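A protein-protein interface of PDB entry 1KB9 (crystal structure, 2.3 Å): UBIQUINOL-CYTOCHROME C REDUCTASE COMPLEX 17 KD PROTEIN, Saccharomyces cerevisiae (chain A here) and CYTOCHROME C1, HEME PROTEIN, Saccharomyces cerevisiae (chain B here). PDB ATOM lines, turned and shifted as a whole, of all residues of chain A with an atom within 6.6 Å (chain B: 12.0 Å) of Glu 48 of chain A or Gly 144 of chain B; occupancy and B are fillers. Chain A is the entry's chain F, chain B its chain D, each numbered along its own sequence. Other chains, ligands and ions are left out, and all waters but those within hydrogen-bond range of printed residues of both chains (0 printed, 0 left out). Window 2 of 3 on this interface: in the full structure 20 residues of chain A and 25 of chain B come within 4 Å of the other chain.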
ATOM      1  N   TYR A  25     -35.166  -6.203   0.545  1.00  0.00           N
ATOM      2  CA  TYR A  25     -34.036  -5.296   0.707  1.00  0.00           C
ATOM      3  C   TYR A  25     -34.361  -4.339   1.848  1.00  0.00           C
ATOM      4  O   TYR A  25     -33.504  -4.035   2.681  1.00  0.00           O
ATOM      5  CB  TYR A  25     -33.747  -4.495  -0.577  1.00  0.00           C
ATOM      6  CG  TYR A  25     -32.764  -3.363  -0.338  1.00  0.00           C
ATOM      7  CD1 TYR A  25     -31.429  -3.630  -0.049  1.00  0.00           C
ATOM      8  CD2 TYR A  25     -33.198  -2.038  -0.263  1.00  0.00           C
ATOM      9  CE1 TYR A  25     -30.554  -2.621   0.326  1.00  0.00           C
ATOM     10  CE2 TYR A  25     -32.325  -1.011   0.111  1.00  0.00           C
ATOM     11  CZ  TYR A  25     -31.005  -1.315   0.410  1.00  0.00           C
ATOM     12  OH  TYR A  25     -30.141  -0.325   0.830  1.00  0.00           O
ATOM     13  N   CYS A  28     -34.096  -5.762   5.239  1.00  0.00           N
ATOM     14  CA  CYS A  28     -32.687  -5.888   5.592  1.00  0.00           C
ATOM     15  C   CYS A  28     -32.155  -4.547   6.078  1.00  0.00           C
ATOM     16  O   CYS A  28     -31.448  -4.483   7.080  1.00  0.00           O
ATOM     17  CB  CYS A  28     -31.858  -6.363   4.392  1.00  0.00           C
ATOM     18  SG  CYS A  28     -30.083  -6.613   4.753  1.00  0.00           S
ATOM     19  N   ARG A  31     -33.326  -3.791   9.629  1.00  0.00           N
ATOM     20  CA  ARG A  31     -32.563  -4.603  10.569  1.00  0.00           C
ATOM     21  C   ARG A  31     -31.149  -4.064  10.797  1.00  0.00           C
ATOM     22  O   ARG A  31     -30.603  -4.184  11.892  1.00  0.00           O
ATOM     23  CB  ARG A  31     -32.521  -6.052  10.066  1.00  0.00           C
ATOM     24  CG  ARG A  31     -31.776  -7.028  10.964  1.00  0.00           C
ATOM     25  CD  ARG A  31     -31.990  -8.480  10.530  1.00  0.00           C
ATOM     26  NE  ARG A  31     -31.476  -8.764   9.190  1.00  0.00           N
ATOM     27  CZ  ARG A  31     -32.238  -9.053   8.136  1.00  0.00           C
ATOM     28  NH1 ARG A  31     -31.678  -9.300   6.957  1.00  0.00           N
ATOM     29  NH2 ARG A  31     -33.560  -9.086   8.254  1.00  0.00           N
ATOM     30  N   VAL A  32     -30.586  -3.419   9.778  1.00  0.00           N
ATOM     31  CA  VAL A  32     -29.235  -2.869   9.862  1.00  0.00           C
ATOM     32  C   VAL A  32     -29.105  -1.599  10.701  1.00  0.00           C
ATOM     33  O   VAL A  32     -28.225  -1.519  11.557  1.00  0.00           O
ATOM     34  CB  VAL A  32     -28.637  -2.622   8.456  1.00  0.00           C
ATOM     35  CG1 VAL A  32     -27.268  -1.958   8.564  1.00  0.00           C
ATOM     36  CG2 VAL A  32     -28.508  -3.935   7.712  1.00  0.00           C
ATOM     37  N   GLN A  35     -29.103  -2.132  14.395  1.00  0.00           N
ATOM     38  CA  GLN A  35     -27.859  -2.670  14.942  1.00  0.00           C
ATOM     39  C   GLN A  35     -26.794  -1.590  15.126  1.00  0.00           C
ATOM     40  O   GLN A  35     -25.906  -1.726  15.971  1.00  0.00           O
ATOM     41  CB  GLN A  35     -27.305  -3.772  14.033  1.00  0.00           C
ATOM     42  CG  GLN A  35     -28.179  -5.013  13.919  1.00  0.00           C
ATOM     43  CD  GLN A  35     -27.567  -6.078  13.021  1.00  0.00           C
ATOM     44  OE1 GLN A  35     -26.380  -6.024  12.689  1.00  0.00           O
ATOM     45  NE2 GLN A  35     -28.377  -7.054  12.627  1.00  0.00           N
ATOM     46  N   GLN A  36     -26.882  -0.530  14.326  1.00  0.00           N
ATOM     47  CA  GLN A  36     -25.925   0.575  14.383  1.00  0.00           C
ATOM     48  C   GLN A  36     -26.118   1.468  15.606  1.00  0.00           C
ATOM     49  O   GLN A  36     -25.147   1.946  16.197  1.00  0.00           O
ATOM     50  CB  GLN A  36     -26.017   1.426  13.113  1.00  0.00           C
ATOM     51  CG  GLN A  36     -25.787   0.655  11.822  1.00  0.00           C
ATOM     52  CD  GLN A  36     -25.779   1.547  10.594  1.00  0.00           C
ATOM     53  OE1 GLN A  36     -25.003   1.331   9.665  1.00  0.00           O
ATOM     54  NE2 GLN A  36     -26.648   2.554  10.583  1.00  0.00           N
ATOM     55  N   TYR A  41     -21.191  -1.105  18.345  1.00  0.00           N
ATOM     56  CA  TYR A  41     -21.264  -1.357  16.910  1.00  0.00           C
ATOM     57  C   TYR A  41     -19.899  -1.231  16.240  1.00  0.00           C
ATOM     58  O   TYR A  41     -19.579  -1.997  15.332  1.00  0.00           O
ATOM     59  CB  TYR A  41     -22.265  -0.411  16.240  1.00  0.00           C
ATOM     60  CG  TYR A  41     -22.425  -0.653  14.753  1.00  0.00           C
ATOM     61  CD1 TYR A  41     -21.945   0.267  13.822  1.00  0.00           C
ATOM     62  CD2 TYR A  41     -23.038  -1.813  14.277  1.00  0.00           C
ATOM     63  CE1 TYR A  41     -22.070   0.040  12.456  1.00  0.00           C
ATOM     64  CE2 TYR A  41     -23.167  -2.050  12.912  1.00  0.00           C
ATOM     65  CZ  TYR A  41     -22.681  -1.120  12.007  1.00  0.00           C
ATOM     66  OH  TYR A  41     -22.802  -1.347  10.655  1.00  0.00           O
ATOM     67  N   HIS A  46     -18.655  -8.270  12.870  1.00  0.00           N
ATOM     68  CA  HIS A  46     -19.723  -9.129  12.370  1.00  0.00           C
ATOM     69  C   HIS A  46     -20.874  -8.261  11.851  1.00  0.00           C
ATOM     70  O   HIS A  46     -22.040  -8.661  11.896  1.00  0.00           O
ATOM     71  CB  HIS A  46     -20.213 -10.037  13.504  1.00  0.00           C
ATOM     72  CG  HIS A  46     -20.626 -11.403  13.054  1.00  0.00           C
ATOM     73  ND1 HIS A  46     -21.856 -11.663  12.487  1.00  0.00           N
ATOM     74  CD2 HIS A  46     -19.978 -12.591  13.107  1.00  0.00           C
ATOM     75  CE1 HIS A  46     -21.948 -12.953  12.213  1.00  0.00           C
ATOM     76  NE2 HIS A  46     -20.823 -13.538  12.579  1.00  0.00           N
ATOM     77  N   LYS A  47     -20.528  -7.075  11.354  1.00  0.00           N
ATOM     78  CA  LYS A  47     -21.501  -6.122  10.829  1.00  0.00           C
ATOM     79  C   LYS A  47     -22.139  -6.634   9.541  1.00  0.00           C
ATOM     80  O   LYS A  47     -21.447  -6.983   8.585  1.00  0.00           O
ATOM     81  CB  LYS A  47     -20.838  -4.767  10.559  1.00  0.00           C
ATOM     82  CG  LYS A  47     -19.868  -4.307  11.639  1.00  0.00           C
ATOM     83  CD  LYS A  47     -19.271  -2.947  11.302  1.00  0.00           C
ATOM     84  CE  LYS A  47     -17.917  -2.744  11.973  1.00  0.00           C
ATOM     85  NZ  LYS A  47     -17.965  -2.926  13.448  1.00  0.00           N
ATOM     86  N   GLU A  48     -23.464  -6.680   9.530  1.00  0.00           N
ATOM     87  CA  GLU A  48     -24.208  -7.144   8.372  1.00  0.00           C
ATOM     88  C   GLU A  48     -24.521  -5.991   7.423  1.00  0.00           C
ATOM     89  O   GLU A  48     -24.767  -4.865   7.859  1.00  0.00           O
ATOM     90  CB  GLU A  48     -25.513  -7.806   8.827  1.00  0.00           C
ATOM     91  CG  GLU A  48     -26.414  -8.287   7.692  1.00  0.00           C
ATOM     92  CD  GLU A  48     -27.747  -8.838   8.177  1.00  0.00           C
ATOM     93  OE1 GLU A  48     -28.079  -8.658   9.369  1.00  0.00           O
ATOM     94  OE2 GLU A  48     -28.472  -9.448   7.363  1.00  0.00           O
ATOM     95  N   ASP A  49     -24.456  -6.268   6.123  1.00  0.00           N
ATOM     96  CA  ASP A  49     -24.777  -5.275   5.106  1.00  0.00           C
ATOM     97  C   ASP A  49     -25.882  -5.855   4.241  1.00  0.00           C
ATOM     98  O   ASP A  49     -26.231  -7.022   4.383  1.00  0.00           O
ATOM     99  CB  ASP A  49     -23.552  -4.891   4.265  1.00  0.00           C
ATOM    100  CG  ASP A  49     -22.937  -6.071   3.534  1.00  0.00           C
ATOM    101  OD1 ASP A  49     -21.779  -6.409   3.861  1.00  0.00           O
ATOM    102  OD2 ASP A  49     -23.588  -6.640   2.626  1.00  0.00           O
ATOM    103  N   CYS A  50     -26.422  -5.053   3.333  1.00  0.00           N
ATOM    104  CA  CYS A  50     -27.507  -5.526   2.488  1.00  0.00           C
ATOM    105  C   CYS A  50     -27.182  -5.575   0.991  1.00  0.00           C
ATOM    106  O   CYS A  50     -28.084  -5.508   0.142  1.00  0.00           O
ATOM    107  CB  CYS A  50     -28.768  -4.703   2.774  1.00  0.00           C
ATOM    108  SG  CYS A  50     -29.263  -4.763   4.535  1.00  0.00           S
ATOM    109  N   GLU A  53     -29.049  -8.544  -0.842  1.00  0.00           N
ATOM    110  CA  GLU A  53     -30.448  -8.209  -1.115  1.00  0.00           C
ATOM    111  C   GLU A  53     -30.516  -7.134  -2.195  1.00  0.00           C
ATOM    112  O   GLU A  53     -31.397  -7.161  -3.054  1.00  0.00           O
ATOM    113  CB  GLU A  53     -31.157  -7.720   0.153  1.00  0.00           C
ATOM    114  CG  GLU A  53     -31.379  -8.789   1.225  1.00  0.00           C
ATOM    115  CD  GLU A  53     -30.127  -9.121   2.025  1.00  0.00           C
ATOM    116  OE1 GLU A  53     -29.128  -8.370   1.944  1.00  0.00           O
ATOM    117  OE2 GLU A  53     -30.148 -10.134   2.756  1.00  0.00           O
ATOM    118  N   THR B   2     -17.388 -13.632  -2.501  1.00  0.00           N
ATOM    119  CA  THR B   2     -18.627 -12.864  -2.293  1.00  0.00           C
ATOM    120  C   THR B   2     -19.037 -12.020  -3.495  1.00  0.00           C
ATOM    121  O   THR B   2     -18.192 -11.528  -4.239  1.00  0.00           O
ATOM    122  CB  THR B   2     -18.578 -11.937  -1.047  1.00  0.00           C
ATOM    123  OG1 THR B   2     -17.610 -10.900  -1.241  1.00  0.00           O
ATOM    124  CG2 THR B   2     -18.239 -12.722   0.205  1.00  0.00           C
ATOM    125  N   ALA B   4     -20.155  -9.041  -3.669  1.00  0.00           N
ATOM    126  CA  ALA B   4     -19.629  -7.682  -3.598  1.00  0.00           C
ATOM    127  C   ALA B   4     -18.230  -7.616  -4.189  1.00  0.00           C
ATOM    128  O   ALA B   4     -17.924  -6.732  -4.990  1.00  0.00           O
ATOM    129  CB  ALA B   4     -19.612  -7.196  -2.152  1.00  0.00           C
ATOM    130  N   GLU B 140     -27.686   6.348  -3.117  1.00  0.00           N
ATOM    131  CA  GLU B 140     -27.160   5.999  -1.804  1.00  0.00           C
ATOM    132  C   GLU B 140     -26.734   4.530  -1.781  1.00  0.00           C
ATOM    133  O   GLU B 140     -27.412   3.676  -2.350  1.00  0.00           O
ATOM    134  CB  GLU B 140     -28.218   6.264  -0.723  1.00  0.00           C
ATOM    135  CG  GLU B 140     -28.416   7.745  -0.389  1.00  0.00           C
ATOM    136  CD  GLU B 140     -29.623   8.004   0.500  1.00  0.00           C
ATOM    137  OE1 GLU B 140     -29.540   7.736   1.722  1.00  0.00           O
ATOM    138  OE2 GLU B 140     -30.652   8.489  -0.029  1.00  0.00           O
ATOM    139  N   PRO B 141     -25.579   4.226  -1.162  1.00  0.00           N
ATOM    140  CA  PRO B 141     -25.082   2.847  -1.077  1.00  0.00           C
ATOM    141  C   PRO B 141     -25.998   1.975  -0.222  1.00  0.00           C
ATOM    142  O   PRO B 141     -26.670   2.476   0.680  1.00  0.00           O
ATOM    143  CB  PRO B 141     -23.709   3.023  -0.419  1.00  0.00           C
ATOM    144  CG  PRO B 141     -23.882   4.250   0.411  1.00  0.00           C
ATOM    145  CD  PRO B 141     -24.628   5.157  -0.531  1.00  0.00           C
ATOM    146  N   PRO B 142     -26.046   0.658  -0.501  1.00  0.00           N
ATOM    147  CA  PRO B 142     -26.896  -0.251   0.273  1.00  0.00           C
ATOM    148  C   PRO B 142     -26.545  -0.220   1.759  1.00  0.00           C
ATOM    149  O   PRO B 142     -25.384  -0.046   2.132  1.00  0.00           O
ATOM    150  CB  PRO B 142     -26.611  -1.614  -0.367  1.00  0.00           C
ATOM    151  CG  PRO B 142     -25.228  -1.468  -0.894  1.00  0.00           C
ATOM    152  CD  PRO B 142     -25.264  -0.090  -1.499  1.00  0.00           C
ATOM    153  N   ALA B 143     -27.567  -0.378   2.594  1.00  0.00           N
ATOM    154  CA  ALA B 143     -27.423  -0.346   4.046  1.00  0.00           C
ATOM    155  C   ALA B 143     -26.305  -1.218   4.603  1.00  0.00           C
ATOM    156  O   ALA B 143     -26.185  -2.388   4.250  1.00  0.00           O
ATOM    157  CB  ALA B 143     -28.745  -0.713   4.701  1.00  0.00           C
ATOM    158  N   GLY B 144     -25.493  -0.631   5.477  1.00  0.00           N
ATOM    159  CA  GLY B 144     -24.407  -1.366   6.097  1.00  0.00           C
ATOM    160  C   GLY B 144     -23.053  -1.167   5.454  1.00  0.00           C
ATOM    161  O   GLY B 144     -22.023  -1.407   6.084  1.00  0.00           O
ATOM    162  N   VAL B 145     -23.049  -0.732   4.200  1.00  0.00           N
ATOM    163  CA  VAL B 145     -21.804  -0.508   3.480  1.00  0.00           C
ATOM    164  C   VAL B 145     -21.074   0.732   3.985  1.00  0.00           C
ATOM    165  O   VAL B 145     -21.578   1.854   3.888  1.00  0.00           O
ATOM    166  CB  VAL B 145     -22.044  -0.399   1.958  1.00  0.00           C
ATOM    167  CG1 VAL B 145     -20.745  -0.087   1.236  1.00  0.00           C
ATOM    168  CG2 VAL B 145     -22.628  -1.695   1.436  1.00  0.00           C
ATOM    169  N   ALA B 146     -19.897   0.502   4.561  1.00  0.00           N
ATOM    170  CA  ALA B 146     -19.057   1.573   5.082  1.00  0.00           C
ATOM    171  C   ALA B 146     -18.139   2.021   3.953  1.00  0.00           C
ATOM    172  O   ALA B 146     -17.091   1.417   3.707  1.00  0.00           O
ATOM    173  CB  ALA B 146     -18.242   1.072   6.269  1.00  0.00           C
ATOM    174  N   LEU B 147     -18.558   3.072   3.259  1.00  0.00           N
ATOM    175  CA  LEU B 147     -17.806   3.608   2.133  1.00  0.00           C
ATOM    176  C   LEU B 147     -16.729   4.596   2.580  1.00  0.00           C
ATOM    177  O   LEU B 147     -17.033   5.606   3.217  1.00  0.00           O
ATOM    178  CB  LEU B 147     -18.774   4.291   1.170  1.00  0.00           C
ATOM    179  CG  LEU B 147     -18.366   4.393  -0.295  1.00  0.00           C
ATOM    180  CD1 LEU B 147     -18.174   2.997  -0.886  1.00  0.00           C
ATOM    181  CD2 LEU B 147     -19.450   5.148  -1.045  1.00  0.00           C
ATOM    182  N   PRO B 148     -15.455   4.319   2.241  1.00  0.00           N
ATOM    183  CA  PRO B 148     -14.315   5.174   2.596  1.00  0.00           C
ATOM    184  C   PRO B 148     -14.468   6.604   2.064  1.00  0.00           C
ATOM    185  O   PRO B 148     -15.140   6.832   1.055  1.00  0.00           O
ATOM    186  CB  PRO B 148     -13.138   4.466   1.920  1.00  0.00           C
ATOM    187  CG  PRO B 148     -13.551   3.034   1.932  1.00  0.00           C
ATOM    188  CD  PRO B 148     -14.996   3.123   1.512  1.00  0.00           C
ATOM    189  N   TYR B 153     -19.871   4.479  -4.442  1.00  0.00           N
ATOM    190  CA  TYR B 153     -20.373   3.132  -4.594  1.00  0.00           C
ATOM    191  C   TYR B 153     -20.957   2.907  -5.978  1.00  0.00           C
ATOM    192  O   TYR B 153     -21.652   3.764  -6.527  1.00  0.00           O
ATOM    193  CB  TYR B 153     -21.412   2.799  -3.523  1.00  0.00           C
ATOM    194  CG  TYR B 153     -21.938   1.383  -3.624  1.00  0.00           C
ATOM    195  CD1 TYR B 153     -21.276   0.325  -2.999  1.00  0.00           C
ATOM    196  CD2 TYR B 153     -23.076   1.094  -4.375  1.00  0.00           C
ATOM    197  CE1 TYR B 153     -21.737  -0.985  -3.124  1.00  0.00           C
ATOM    198  CE2 TYR B 153     -23.542  -0.207  -4.510  1.00  0.00           C
ATOM    199  CZ  TYR B 153     -22.867  -1.238  -3.880  1.00  0.00           C
ATOM    200  OH  TYR B 153     -23.335  -2.516  -4.006  1.00  0.00           O
ATOM    201  N   GLY B 159     -15.709  -4.986  -5.741  1.00  0.00           N
ATOM    202  CA  GLY B 159     -15.476  -4.412  -4.425  1.00  0.00           C
ATOM    203  C   GLY B 159     -16.413  -3.252  -4.112  1.00  0.00           C
ATOM    204  O   GLY B 159     -16.390  -2.717  -2.999  1.00  0.00           O
ATOM    205  N   GLY B 160     -17.192  -2.838  -5.115  1.00  0.00           N
ATOM    206  CA  GLY B 160     -18.159  -1.762  -4.966  1.00  0.00           C
ATOM    207  C   GLY B 160     -17.656  -0.344  -4.753  1.00  0.00           C
ATOM    208  O   GLY B 160     -18.379   0.615  -5.036  1.00  0.00           O
ATOM    209  N   SER B 161     -16.427  -0.204  -4.263  1.00  0.00           N
ATOM    210  CA  SER B 161     -15.850   1.105  -3.992  1.00  0.00           C
ATOM    211  C   SER B 161     -14.965   1.623  -5.127  1.00  0.00           C
ATOM    212  O   SER B 161     -13.829   1.183  -5.295  1.00  0.00           O
ATOM    213  CB  SER B 161     -15.073   1.053  -2.676  1.00  0.00           C
ATOM    214  OG  SER B 161     -14.426   2.282  -2.417  1.00  0.00           O
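N of Ala 143 of chain B sits at hydrogen-bond distance from OH of Tyr 25 of chain A (3.1 Å). O of Ala 143 of chain B is in hydrogen-bond range of N of Cys 50 of chain A (2.8 Å).
SG of Cys 28 of chain A is disulfide-bonded to SG of Cys 50 of chain A, 2.0 Å away. OE2 of Glu 48 of chain A is in salt-bridge range of NH1 of Arg 31 of chain A, at 3.2 Å.
Among the printed residues, merely in contact across the chains: Tyr 25 of chain A with Pro 142 of chain B (3.3 Å), Val 32 of chain A with Gly 144 of chain B (3.8 Å), Glu 48 of chain A with Gly 144 of chain B (3.9 Å), Asp 49 of chain A with Ala 143 of chain B (3.3 Å) and Asp 49 of chain A with Gly 144 of chain B (3.9 Å).
Printed residues of chain B within 4 Å of Tyr 25 of chain A: Pro 142 (3.3 Å) and Ala 143 (3.1 Å). No residue of chain B comes within 4 Å of Arg 31 of chain A. Val 32 of chain A touches one residue of chain B. No residue of chain B comes within 4 Å of Lys 47 of chain A. Glu 48 of chain A touches just one residue of chain B: Gly 144 (3.9 Å). Asp 49 of chain A touches just these residues of chain B: Ala 143 and Gly 144. Of the printed residues of chain A, Pro 142 of chain B touches Tyr 25. Of the printed residues of chain A, Ala 143 of chain B touches Tyr 25, Asp 49 and Cys 50. Of chain A, only Val 32, Glu 48 and Asp 49 come within 4 Å of Gly 144 of chain B. Pro 148 of chain B touches none of the printed residues of chain A. The nearest printed residue of chain B that does not touch Tyr 25 of chain A is Pro 141 of chain B (4.5 Å).
Printed residues of chain A that touch a printed residue of chain B: Tyr 25, Val 32, Glu 48, Asp 49 and Cys 50. Hydrophobic or aromatic side chains of chain A within 4 Å of the printed part of chain B: Tyr 25 and Val 32. Among the printed residues, no Asp or Glu carboxylate lies within 4 Å of a Lys or Arg side-chain nitrogen of the other chain.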
